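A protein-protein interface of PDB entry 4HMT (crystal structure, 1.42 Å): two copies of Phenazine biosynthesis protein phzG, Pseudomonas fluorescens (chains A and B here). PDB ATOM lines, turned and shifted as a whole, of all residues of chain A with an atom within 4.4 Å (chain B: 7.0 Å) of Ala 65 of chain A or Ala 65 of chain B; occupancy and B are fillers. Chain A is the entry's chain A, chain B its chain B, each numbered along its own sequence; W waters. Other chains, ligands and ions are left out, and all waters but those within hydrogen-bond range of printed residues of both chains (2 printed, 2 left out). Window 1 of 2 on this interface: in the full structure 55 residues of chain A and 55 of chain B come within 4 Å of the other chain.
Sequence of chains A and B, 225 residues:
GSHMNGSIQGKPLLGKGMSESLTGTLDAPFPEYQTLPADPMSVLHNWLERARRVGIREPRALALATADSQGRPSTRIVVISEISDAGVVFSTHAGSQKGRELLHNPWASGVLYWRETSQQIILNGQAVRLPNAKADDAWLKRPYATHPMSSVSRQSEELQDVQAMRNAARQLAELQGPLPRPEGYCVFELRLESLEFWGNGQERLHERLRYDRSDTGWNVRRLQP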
ATOM      1  N   ALA A  63      -9.538   2.012 -13.983  1.00  0.00           N
ATOM      2  CA  ALA A  63      -9.632   2.147 -15.426  1.00  0.00           C
ATOM      3  C   ALA A  63     -10.798   3.086 -15.714  1.00  0.00           C
ATOM      4  O   ALA A  63     -11.947   2.704 -15.588  1.00  0.00           O
ATOM      5  CB  ALA A  63      -9.799   0.822 -16.085  1.00  0.00           C
ATOM      6  N   LEU A  64     -10.449   4.332 -16.045  1.00  0.00           N
ATOM      7  CA  LEU A  64     -11.392   5.441 -16.149  1.00  0.00           C
ATOM      8  C   LEU A  64     -11.737   5.716 -17.596  1.00  0.00           C
ATOM      9  O   LEU A  64     -10.841   6.011 -18.403  1.00  0.00           O
ATOM     10  CB  LEU A  64     -10.801   6.721 -15.500  1.00  0.00           C
ATOM     11  CG  LEU A  64     -11.735   7.946 -15.594  1.00  0.00           C
ATOM     12  CD1 LEU A  64     -12.892   7.788 -14.667  1.00  0.00           C
ATOM     13  CD2 LEU A  64     -10.912   9.217 -15.319  1.00  0.00           C
ATOM     14  N   ALA A  65     -13.019   5.684 -17.895  1.00  0.00           N
ATOM     15  CA  ALA A  65     -13.567   5.967 -19.223  1.00  0.00           C
ATOM     16  C   ALA A  65     -14.265   7.288 -19.237  1.00  0.00           C
ATOM     17  O   ALA A  65     -15.083   7.595 -18.373  1.00  0.00           O
ATOM     18  CB  ALA A  65     -14.583   4.855 -19.634  1.00  0.00           C
ATOM     19  N   THR A  66     -13.957   8.050 -20.275  1.00  0.00           N
ATOM     20  CA  THR A  66     -14.623   9.256 -20.627  1.00  0.00           C
ATOM     21  C   THR A  66     -15.074   9.110 -22.067  1.00  0.00           C
ATOM     22  O   THR A  66     -14.726   8.139 -22.727  1.00  0.00           O
ATOM     23  CB  THR A  66     -13.649  10.454 -20.483  1.00  0.00           C
ATOM     24  OG1 THR A  66     -12.456  10.254 -21.220  1.00  0.00           O
ATOM     25  CG2 THR A  66     -13.221  10.634 -19.018  1.00  0.00           C
ATOM     26  N   PRO A  73     -15.731   6.440 -26.623  1.00  0.00           N
ATOM     27  CA  PRO A  73     -15.021   6.354 -25.340  1.00  0.00           C
ATOM     28  C   PRO A  73     -13.502   6.371 -25.501  1.00  0.00           C
ATOM     29  O   PRO A  73     -12.928   5.996 -26.537  1.00  0.00           O
ATOM     30  CB  PRO A  73     -15.472   4.976 -24.774  1.00  0.00           C
ATOM     31  CG  PRO A  73     -16.663   4.598 -25.569  1.00  0.00           C
ATOM     32  CD  PRO A  73     -16.502   5.218 -26.905  1.00  0.00           C
ATOM     33  N   SER A  74     -12.846   6.774 -24.423  1.00  0.00           N
ATOM     34  CA  SER A  74     -11.404   6.635 -24.241  1.00  0.00           C
ATOM     35  C   SER A  74     -11.177   6.167 -22.829  1.00  0.00           C
ATOM     36  O   SER A  74     -12.009   6.400 -21.956  1.00  0.00           O
ATOM     37  CB  SER A  74     -10.658   7.946 -24.518  1.00  0.00           C
ATOM     38  OG  SER A  74     -11.089   8.959 -23.645  1.00  0.00           O
ATOM     39  N   THR A  75     -10.078   5.468 -22.614  1.00  0.00           N
ATOM     40  CA  THR A  75      -9.734   4.865 -21.312  1.00  0.00           C
ATOM     41  C   THR A  75      -8.285   5.043 -20.970  1.00  0.00           C
ATOM     42  O   THR A  75      -7.438   5.280 -21.854  1.00  0.00           O
ATOM     43  CB  THR A  75     -10.058   3.355 -21.254  1.00  0.00           C
ATOM     44  OG1 THR A  75      -9.311   2.663 -22.304  1.00  0.00           O
ATOM     45  CG2 THR A  75     -11.514   3.074 -21.429  1.00  0.00           C
ATOM     46  N   ARG A  76      -7.990   4.971 -19.665  1.00  0.00           N
ATOM     47  CA  ARG A  76      -6.648   5.014 -19.099  1.00  0.00           C
ATOM     48  C   ARG A  76      -6.762   4.685 -17.641  1.00  0.00           C
ATOM     49  O   ARG A  76      -7.821   4.815 -17.062  1.00  0.00           O
ATOM     50  CB  ARG A  76      -5.960   6.385 -19.296  1.00  0.00           C
ATOM     51  CG  ARG A  76      -6.476   7.454 -18.340  1.00  0.00           C
ATOM     52  CD  ARG A  76      -7.892   7.853 -18.633  1.00  0.00           C
ATOM     53  NE  ARG A  76      -8.004   8.472 -19.917  1.00  0.00           N
ATOM     54  CZ  ARG A  76      -9.134   8.770 -20.510  1.00  0.00           C
ATOM     55  NH1 ARG A  76      -9.095   9.474 -21.632  1.00  0.00           N
ATOM     56  NH2 ARG A  76     -10.298   8.441 -20.026  1.00  0.00           N
ATOM     57  N   ALA A 108     -18.709   9.764 -16.766  1.00  0.00           N
ATOM     58  CA  ALA A 108     -17.570   8.891 -16.763  1.00  0.00           C
ATOM     59  C   ALA A 108     -17.930   7.579 -16.088  1.00  0.00           C
ATOM     60  O   ALA A 108     -18.952   7.487 -15.366  1.00  0.00           O
ATOM     61  CB  ALA A 108     -16.379   9.568 -16.067  1.00  0.00           C
ATOM     62  N   SER A 109     -17.104   6.583 -16.288  1.00  0.00           N
ATOM     63  CA  SER A 109     -17.269   5.302 -15.623  1.00  0.00           C
ATOM     64  C   SER A 109     -15.904   4.770 -15.380  1.00  0.00           C
ATOM     65  O   SER A 109     -15.037   4.908 -16.240  1.00  0.00           O
ATOM     66  CB  SER A 109     -18.027   4.318 -16.544  1.00  0.00           C
ATOM     67  OG  SER A 109     -18.147   3.060 -15.897  1.00  0.00           O
ATOM     68  N   LEU B  62      -9.257  -7.044 -19.971  1.00  0.00           N
ATOM     69  CA  LEU B  62      -9.468  -5.746 -20.587  1.00  0.00           C
ATOM     70  C   LEU B  62     -10.577  -4.962 -19.917  1.00  0.00           C
ATOM     71  O   LEU B  62     -11.728  -5.448 -19.869  1.00  0.00           O
ATOM     72  CB  LEU B  62      -9.801  -5.966 -22.067  1.00  0.00           C
ATOM     73  CG  LEU B  62      -9.935  -4.712 -22.927  1.00  0.00           C
ATOM     74  CD1 LEU B  62      -8.530  -4.078 -23.177  1.00  0.00           C
ATOM     75  CD2 LEU B  62     -10.588  -5.082 -24.261  1.00  0.00           C
ATOM     76  N   ALA B  63     -10.275  -3.745 -19.444  1.00  0.00           N
ATOM     77  CA  ALA B  63     -11.305  -2.869 -18.915  1.00  0.00           C
ATOM     78  C   ALA B  63     -11.913  -2.187 -20.131  1.00  0.00           C
ATOM     79  O   ALA B  63     -11.300  -1.273 -20.707  1.00  0.00           O
ATOM     80  CB  ALA B  63     -10.738  -1.887 -17.934  1.00  0.00           C
ATOM     81  N   LEU B  64     -13.095  -2.639 -20.530  1.00  0.00           N
ATOM     82  CA  LEU B  64     -13.726  -2.253 -21.774  1.00  0.00           C
ATOM     83  C   LEU B  64     -14.791  -1.228 -21.533  1.00  0.00           C
ATOM     84  O   LEU B  64     -15.740  -1.480 -20.747  1.00  0.00           O
ATOM     85  CB  LEU B  64     -14.354  -3.490 -22.447  1.00  0.00           C
ATOM     86  CG  LEU B  64     -15.120  -3.174 -23.741  1.00  0.00           C
ATOM     87  CD1 LEU B  64     -14.120  -2.823 -24.833  1.00  0.00           C
ATOM     88  CD2 LEU B  64     -16.023  -4.339 -24.168  1.00  0.00           C
ATOM     89  N   ALA B  65     -14.683  -0.085 -22.213  1.00  0.00           N
ATOM     90  CA  ALA B  65     -15.656   1.002 -22.101  1.00  0.00           C
ATOM     91  C   ALA B  65     -16.498   1.095 -23.359  1.00  0.00           C
ATOM     92  O   ALA B  65     -15.985   1.024 -24.493  1.00  0.00           O
ATOM     93  CB  ALA B  65     -14.969   2.337 -21.929  1.00  0.00           C
ATOM     94  N   THR B  66     -17.786   1.230 -23.151  1.00  0.00           N
ATOM     95  CA  THR B  66     -18.731   1.505 -24.209  1.00  0.00           C
ATOM     96  C   THR B  66     -19.513   2.734 -23.797  1.00  0.00           C
ATOM     97  O   THR B  66     -19.302   3.242 -22.697  1.00  0.00           O
ATOM     98  CB  THR B  66     -19.710   0.307 -24.372  1.00  0.00           C
ATOM     99  OG1 THR B  66     -20.288  -0.024 -23.126  1.00  0.00           O
ATOM    100  CG2 THR B  66     -18.939  -0.926 -24.818  1.00  0.00           C
ATOM    101  N   ALA B  67     -20.391   3.237 -24.654  1.00  0.00           N
ATOM    102  CA  ALA B  67     -21.195   4.402 -24.270  1.00  0.00           C
ATOM    103  C   ALA B  67     -22.656   4.296 -24.683  1.00  0.00           C
ATOM    104  O   ALA B  67     -22.975   3.636 -25.678  1.00  0.00           O
ATOM    105  CB  ALA B  67     -20.591   5.667 -24.755  1.00  0.00           C
ATOM    106  N   PRO B  73     -20.400   6.857 -20.579  1.00  0.00           N
ATOM    107  CA  PRO B  73     -19.642   5.616 -20.605  1.00  0.00           C
ATOM    108  C   PRO B  73     -20.084   4.627 -19.546  1.00  0.00           C
ATOM    109  O   PRO B  73     -20.639   4.982 -18.486  1.00  0.00           O
ATOM    110  CB  PRO B  73     -18.211   6.038 -20.257  1.00  0.00           C
ATOM    111  CG  PRO B  73     -18.158   7.460 -20.504  1.00  0.00           C
ATOM    112  CD  PRO B  73     -19.516   8.007 -20.230  1.00  0.00           C
ATOM    113  N   SER B  74     -19.823   3.360 -19.854  1.00  0.00           N
ATOM    114  CA  SER B  74     -19.914   2.271 -18.870  1.00  0.00           C
ATOM    115  C   SER B  74     -18.694   1.400 -19.053  1.00  0.00           C
ATOM    116  O   SER B  74     -18.126   1.334 -20.136  1.00  0.00           O
ATOM    117  CB  SER B  74     -21.181   1.443 -18.980  1.00  0.00           C
ATOM    118  OG  SER B  74     -21.290   0.876 -20.265  1.00  0.00           O
ATOM    119  N   THR B  75     -18.298   0.689 -18.021  1.00  0.00           N
ATOM    120  CA  THR B  75     -17.073  -0.122 -18.034  1.00  0.00           C
ATOM    121  C   THR B  75     -17.286  -1.459 -17.348  1.00  0.00           C
ATOM    122  O   THR B  75     -18.191  -1.577 -16.518  1.00  0.00           O
ATOM    123  CB  THR B  75     -15.933   0.584 -17.331  1.00  0.00           C
ATOM    124  OG1 THR B  75     -16.262   0.916 -15.981  1.00  0.00           O
ATOM    125  CG2 THR B  75     -15.492   1.813 -18.091  1.00  0.00           C
ATOM    126  N   ARG B  76     -16.455  -2.431 -17.673  1.00  0.00           N
ATOM    127  CA  ARG B  76     -16.425  -3.732 -17.007  1.00  0.00           C
ATOM    128  C   ARG B  76     -15.215  -4.449 -17.566  1.00  0.00           C
ATOM    129  O   ARG B  76     -14.679  -4.070 -18.597  1.00  0.00           O
ATOM    130  CB  ARG B  76     -17.678  -4.577 -17.329  1.00  0.00           C
ATOM    131  CG  ARG B  76     -17.720  -5.170 -18.669  1.00  0.00           C
ATOM    132  CD  ARG B  76     -17.879  -4.168 -19.804  1.00  0.00           C
ATOM    133  NE  ARG B  76     -19.157  -3.433 -19.672  1.00  0.00           N
ATOM    134  CZ  ARG B  76     -19.512  -2.349 -20.339  1.00  0.00           C
ATOM    135  NH1 ARG B  76     -20.763  -1.935 -20.208  1.00  0.00           N
ATOM    136  NH2 ARG B  76     -18.677  -1.696 -21.131  1.00  0.00           N
ATOM    137  N   LYS B  98     -23.231  -3.847 -22.247  1.00  0.00           N
ATOM    138  CA  LYS B  98     -22.195  -3.556 -23.261  1.00  0.00           C
ATOM    139  C   LYS B  98     -22.710  -3.969 -24.656  1.00  0.00           C
ATOM    140  O   LYS B  98     -22.438  -3.291 -25.631  1.00  0.00           O
ATOM    141  CB  LYS B  98     -20.856  -4.210 -22.927  1.00  0.00           C
ATOM    142  CG  LYS B  98     -20.740  -5.672 -23.431  1.00  0.00           C
ATOM    143  CD  LYS B  98     -19.548  -6.423 -22.863  1.00  0.00           C
ATOM    144  CE  LYS B  98     -19.773  -6.792 -21.386  1.00  0.00           C
ATOM    145  NZ  LYS B  98     -21.047  -7.538 -21.157  1.00  0.00           N
ATOM    146  N   GLU B 101     -25.225  -1.438 -25.840  1.00  0.00           N
ATOM    147  CA  GLU B 101     -24.534  -0.178 -26.188  1.00  0.00           C
ATOM    148  C   GLU B 101     -23.774  -0.298 -27.499  1.00  0.00           C
ATOM    149  O   GLU B 101     -23.866   0.598 -28.334  1.00  0.00           O
ATOM    150  CB  GLU B 101     -23.638   0.312 -25.019  1.00  0.00           C
ATOM    151  CG  GLU B 101     -24.491   0.807 -23.837  1.00  0.00           C
ATOM    152  CD  GLU B 101     -23.763   1.421 -22.663  1.00  0.00           C
ATOM    153  OE1 GLU B 101     -22.507   1.473 -22.654  1.00  0.00           O
ATOM    154  OE2 GLU B 101     -24.500   1.900 -21.736  1.00  0.00           O
ATOM    155  N   LEU B 102     -23.044  -1.381 -27.712  1.00  0.00           N
ATOM    156  CA  LEU B 102     -22.264  -1.556 -28.925  1.00  0.00           C
ATOM    157  C   LEU B 102     -23.105  -1.659 -30.187  1.00  0.00           C
ATOM    158  O   LEU B 102     -22.678  -1.316 -31.269  1.00  0.00           O
ATOM    159  CB  LEU B 102     -21.392  -2.820 -28.790  1.00  0.00           C
ATOM    160  CG  LEU B 102     -20.214  -2.608 -27.880  1.00  0.00           C
ATOM    161  CD1 LEU B 102     -19.511  -3.929 -27.637  1.00  0.00           C
ATOM    162  CD2 LEU B 102     -19.220  -1.573 -28.477  1.00  0.00           C
ATOM    163  N   TRP B 107     -18.419   2.362 -31.149  1.00  0.00           N
ATOM    164  CA  TRP B 107     -17.103   2.812 -30.639  1.00  0.00           C
ATOM    165  C   TRP B 107     -16.879   2.364 -29.198  1.00  0.00           C
ATOM    166  O   TRP B 107     -17.765   2.499 -28.339  1.00  0.00           O
ATOM    167  CB  TRP B 107     -17.024   4.334 -30.721  1.00  0.00           C
ATOM    168  CG  TRP B 107     -16.821   4.820 -32.142  1.00  0.00           C
ATOM    169  CD1 TRP B 107     -17.804   5.165 -33.074  1.00  0.00           C
ATOM    170  CD2 TRP B 107     -15.568   4.949 -32.829  1.00  0.00           C
ATOM    171  NE1 TRP B 107     -17.207   5.534 -34.248  1.00  0.00           N
ATOM    172  CE2 TRP B 107     -15.844   5.410 -34.136  1.00  0.00           C
ATOM    173  CE3 TRP B 107     -14.235   4.763 -32.438  1.00  0.00           C
ATOM    174  CZ2 TRP B 107     -14.817   5.686 -35.062  1.00  0.00           C
ATOM    175  CZ3 TRP B 107     -13.217   5.036 -33.372  1.00  0.00           C
ATOM    176  CH2 TRP B 107     -13.533   5.482 -34.671  1.00  0.00           C
ATOM    177  N   ALA B 108     -15.666   1.895 -28.949  1.00  0.00           N
ATOM    178  CA  ALA B 108     -15.283   1.388 -27.648  1.00  0.00           C
ATOM    179  C   ALA B 108     -13.819   1.684 -27.395  1.00  0.00           C
ATOM    180  O   ALA B 108     -13.041   1.974 -28.343  1.00  0.00           O
ATOM    181  CB  ALA B 108     -15.560  -0.097 -27.523  1.00  0.00           C
ATOM    182  N   SER B 109     -13.428   1.598 -26.120  1.00  0.00           N
ATOM    183  CA  SER B 109     -12.027   1.711 -25.764  1.00  0.00           C
ATOM    184  C   SER B 109     -11.771   0.755 -24.638  1.00  0.00           C
ATOM    185  O   SER B 109     -12.621   0.636 -23.720  1.00  0.00           O
ATOM    186  CB  SER B 109     -11.736   3.145 -25.310  1.00  0.00           C
ATOM    187  OG  SER B 109     -10.397   3.296 -24.861  1.00  0.00           O
ATOM    188  N   GLY B 110     -10.612   0.092 -24.627  1.00  0.00           N
ATOM    189  CA  GLY B 110     -10.252  -0.783 -23.533  1.00  0.00           C
ATOM    190  C   GLY B 110      -8.831  -0.535 -23.094  1.00  0.00           C
ATOM    191  O   GLY B 110      -7.972  -0.178 -23.901  1.00  0.00           O
ATOM    192  N   VAL B 111      -8.573  -0.774 -21.833  1.00  0.00           N
ATOM    193  CA  VAL B 111      -7.229  -0.687 -21.296  1.00  0.00           C
ATOM    194  C   VAL B 111      -6.794  -1.963 -20.587  1.00  0.00           C
ATOM    195  O   VAL B 111      -7.552  -2.558 -19.806  1.00  0.00           O
ATOM    196  CB  VAL B 111      -7.074   0.523 -20.368  1.00  0.00           C
ATOM    197  CG1 VAL B 111      -8.099   0.576 -19.221  1.00  0.00           C
ATOM    198  CG2 VAL B 111      -5.649   0.629 -19.796  1.00  0.00           C
HETATM  199  O   HOH W   1     -13.532   4.829 -28.971  1.00  0.00           O
HETATM  200  O   HOH W   2     -21.323   7.361 -17.111  1.00  0.00           O
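The side-chain hydroxyl (OG1) of Thr 75 of chain A is in hydrogen-bond range of the side-chain hydroxyl (OG) of Ser 109 of chain B, at 2.8 Å. OG of Ser 109 of chain A is in hydrogen-bond range of OG1 of Thr 75 of chain B (2.9 Å).
OG1 of Thr 66 of chain A sits at hydrogen-bond distance from NH2 of Arg 76 of chain A, at 3.1 Å. The guanidinium group (NH1) of Arg 76 of chain A is in hydrogen-bond range of the side-chain hydroxyl (OG) of Ser 74 of chain A. The backbone NH of Ala 65 of chain B sits at hydrogen-bond distance from the backbone carbonyl oxygen of Ser 109 of chain B (2.7 Å). The backbone carbonyl oxygen of Thr 66 of chain B is in hydrogen-bond range of the backbone NH of Ser 74 of chain B (2.9 Å). The side-chain hydroxyl (OG1) of Thr 66 of chain B is in hydrogen-bond range of the guanidinium group (NH2) of Arg 76 of chain B (3.1 Å). The side-chain hydroxyl of Thr 66 of chain B lies within hydrogen-bond range of the side-chain carboxylate of Glu 101 of chain B (2.7 Å).
Ala 65 of chain A touches Ala 65 of chain B. Ala 65 of chain A touches Pro 73 of chain B. Ala 65 of chain A touches Thr 75 of chain B (CB to CG2, 3.5 Å). Thr 66 of chain A touches Pro 73 of chain B (C to CG, 3.8 Å). Pro 73 of chain A touches Ala 65 of chain B (CG to O, 3.8 Å). CG of Pro 73 of chain A touches C of Thr 66 of chain B, at 3.8 Å. Thr 75 of chain A touches Ala 65 of chain B (CG2 to CB, 3.6 Å). Val 111 of chain B touches Thr 75 of chain A. N of Ala 108 of chain A touches CD of Pro 73 of chain B, 3.97 Å away. Ser 109 of chain A touches Ser 74 of chain B.
Ala 65 of chain A touches three residues of chain B. Printed residues of chain B within 4 Å of Thr 66 of chain A: Pro 73. Leu 62 of chain B touches none of the printed residues of chain A. Ala 65 of chain B touches just these residues of chain A: Ala 65 (3.4 Å), Pro 73 (3.8 Å) and Thr 75 (3.6 Å). Leu 102 of chain B touches none of the printed residues of chain A. Of the printed residues of chain A, Ser 109 of chain B touches Pro 73, Ser 74 and Thr 75. The nearest residue of chain B that does not touch Ala 65 of chain A is Ser 74 of chain B (5.0 Å). The nearest printed residue of chain A that does not touch Ala 65 of chain B is Ser 74 of chain A (5.0 Å). The nearest printed residue of chain A that does not touch Ser 74 of chain B is Ala 65 of chain A (5.0 Å).
Of the 18 printed residues of chain B, 11 touch a printed residue of chain A. Hydrophobic or aromatic side chains of chain B that line the printed part of chain A: Ala 63, Ala 65, Pro 73, Trp 107 and Val 111. Of the 10 printed residues of chain A, 8 touch a printed residue of chain B. Among the printed residues, 20 pairs touch across the chains.
Ala 65 of chain B touches its own counterpart, Ala 65 of chain A. Ala 65 of chain A touches Thr 75 of chain B, and with the chains exchanged Thr 75 of chain A touches Ala 65 of chain B. Thr 66 of chain A touches Pro 73 of chain B, and with the chains exchanged Pro 73 of chain A touches Thr 66 of chain B. Thr 75 of chain A touches Ser 109 of chain B, and with the chains exchanged Ser 109 of chain A touches Thr 75 of chain B. 10 positions are printed for both chains. Of the 20 pairs that touch across the chains among the printed residues, 16 have their exchanged pair printed and touching as well.
Water W1 lies within hydrogen-bond range of O of Pro 73 of chain A and O of Ala 108 of chain B. Water W2 lies within hydrogen-bond range of O of Pro 73 of chain B and O of Ala 108 of chain A.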
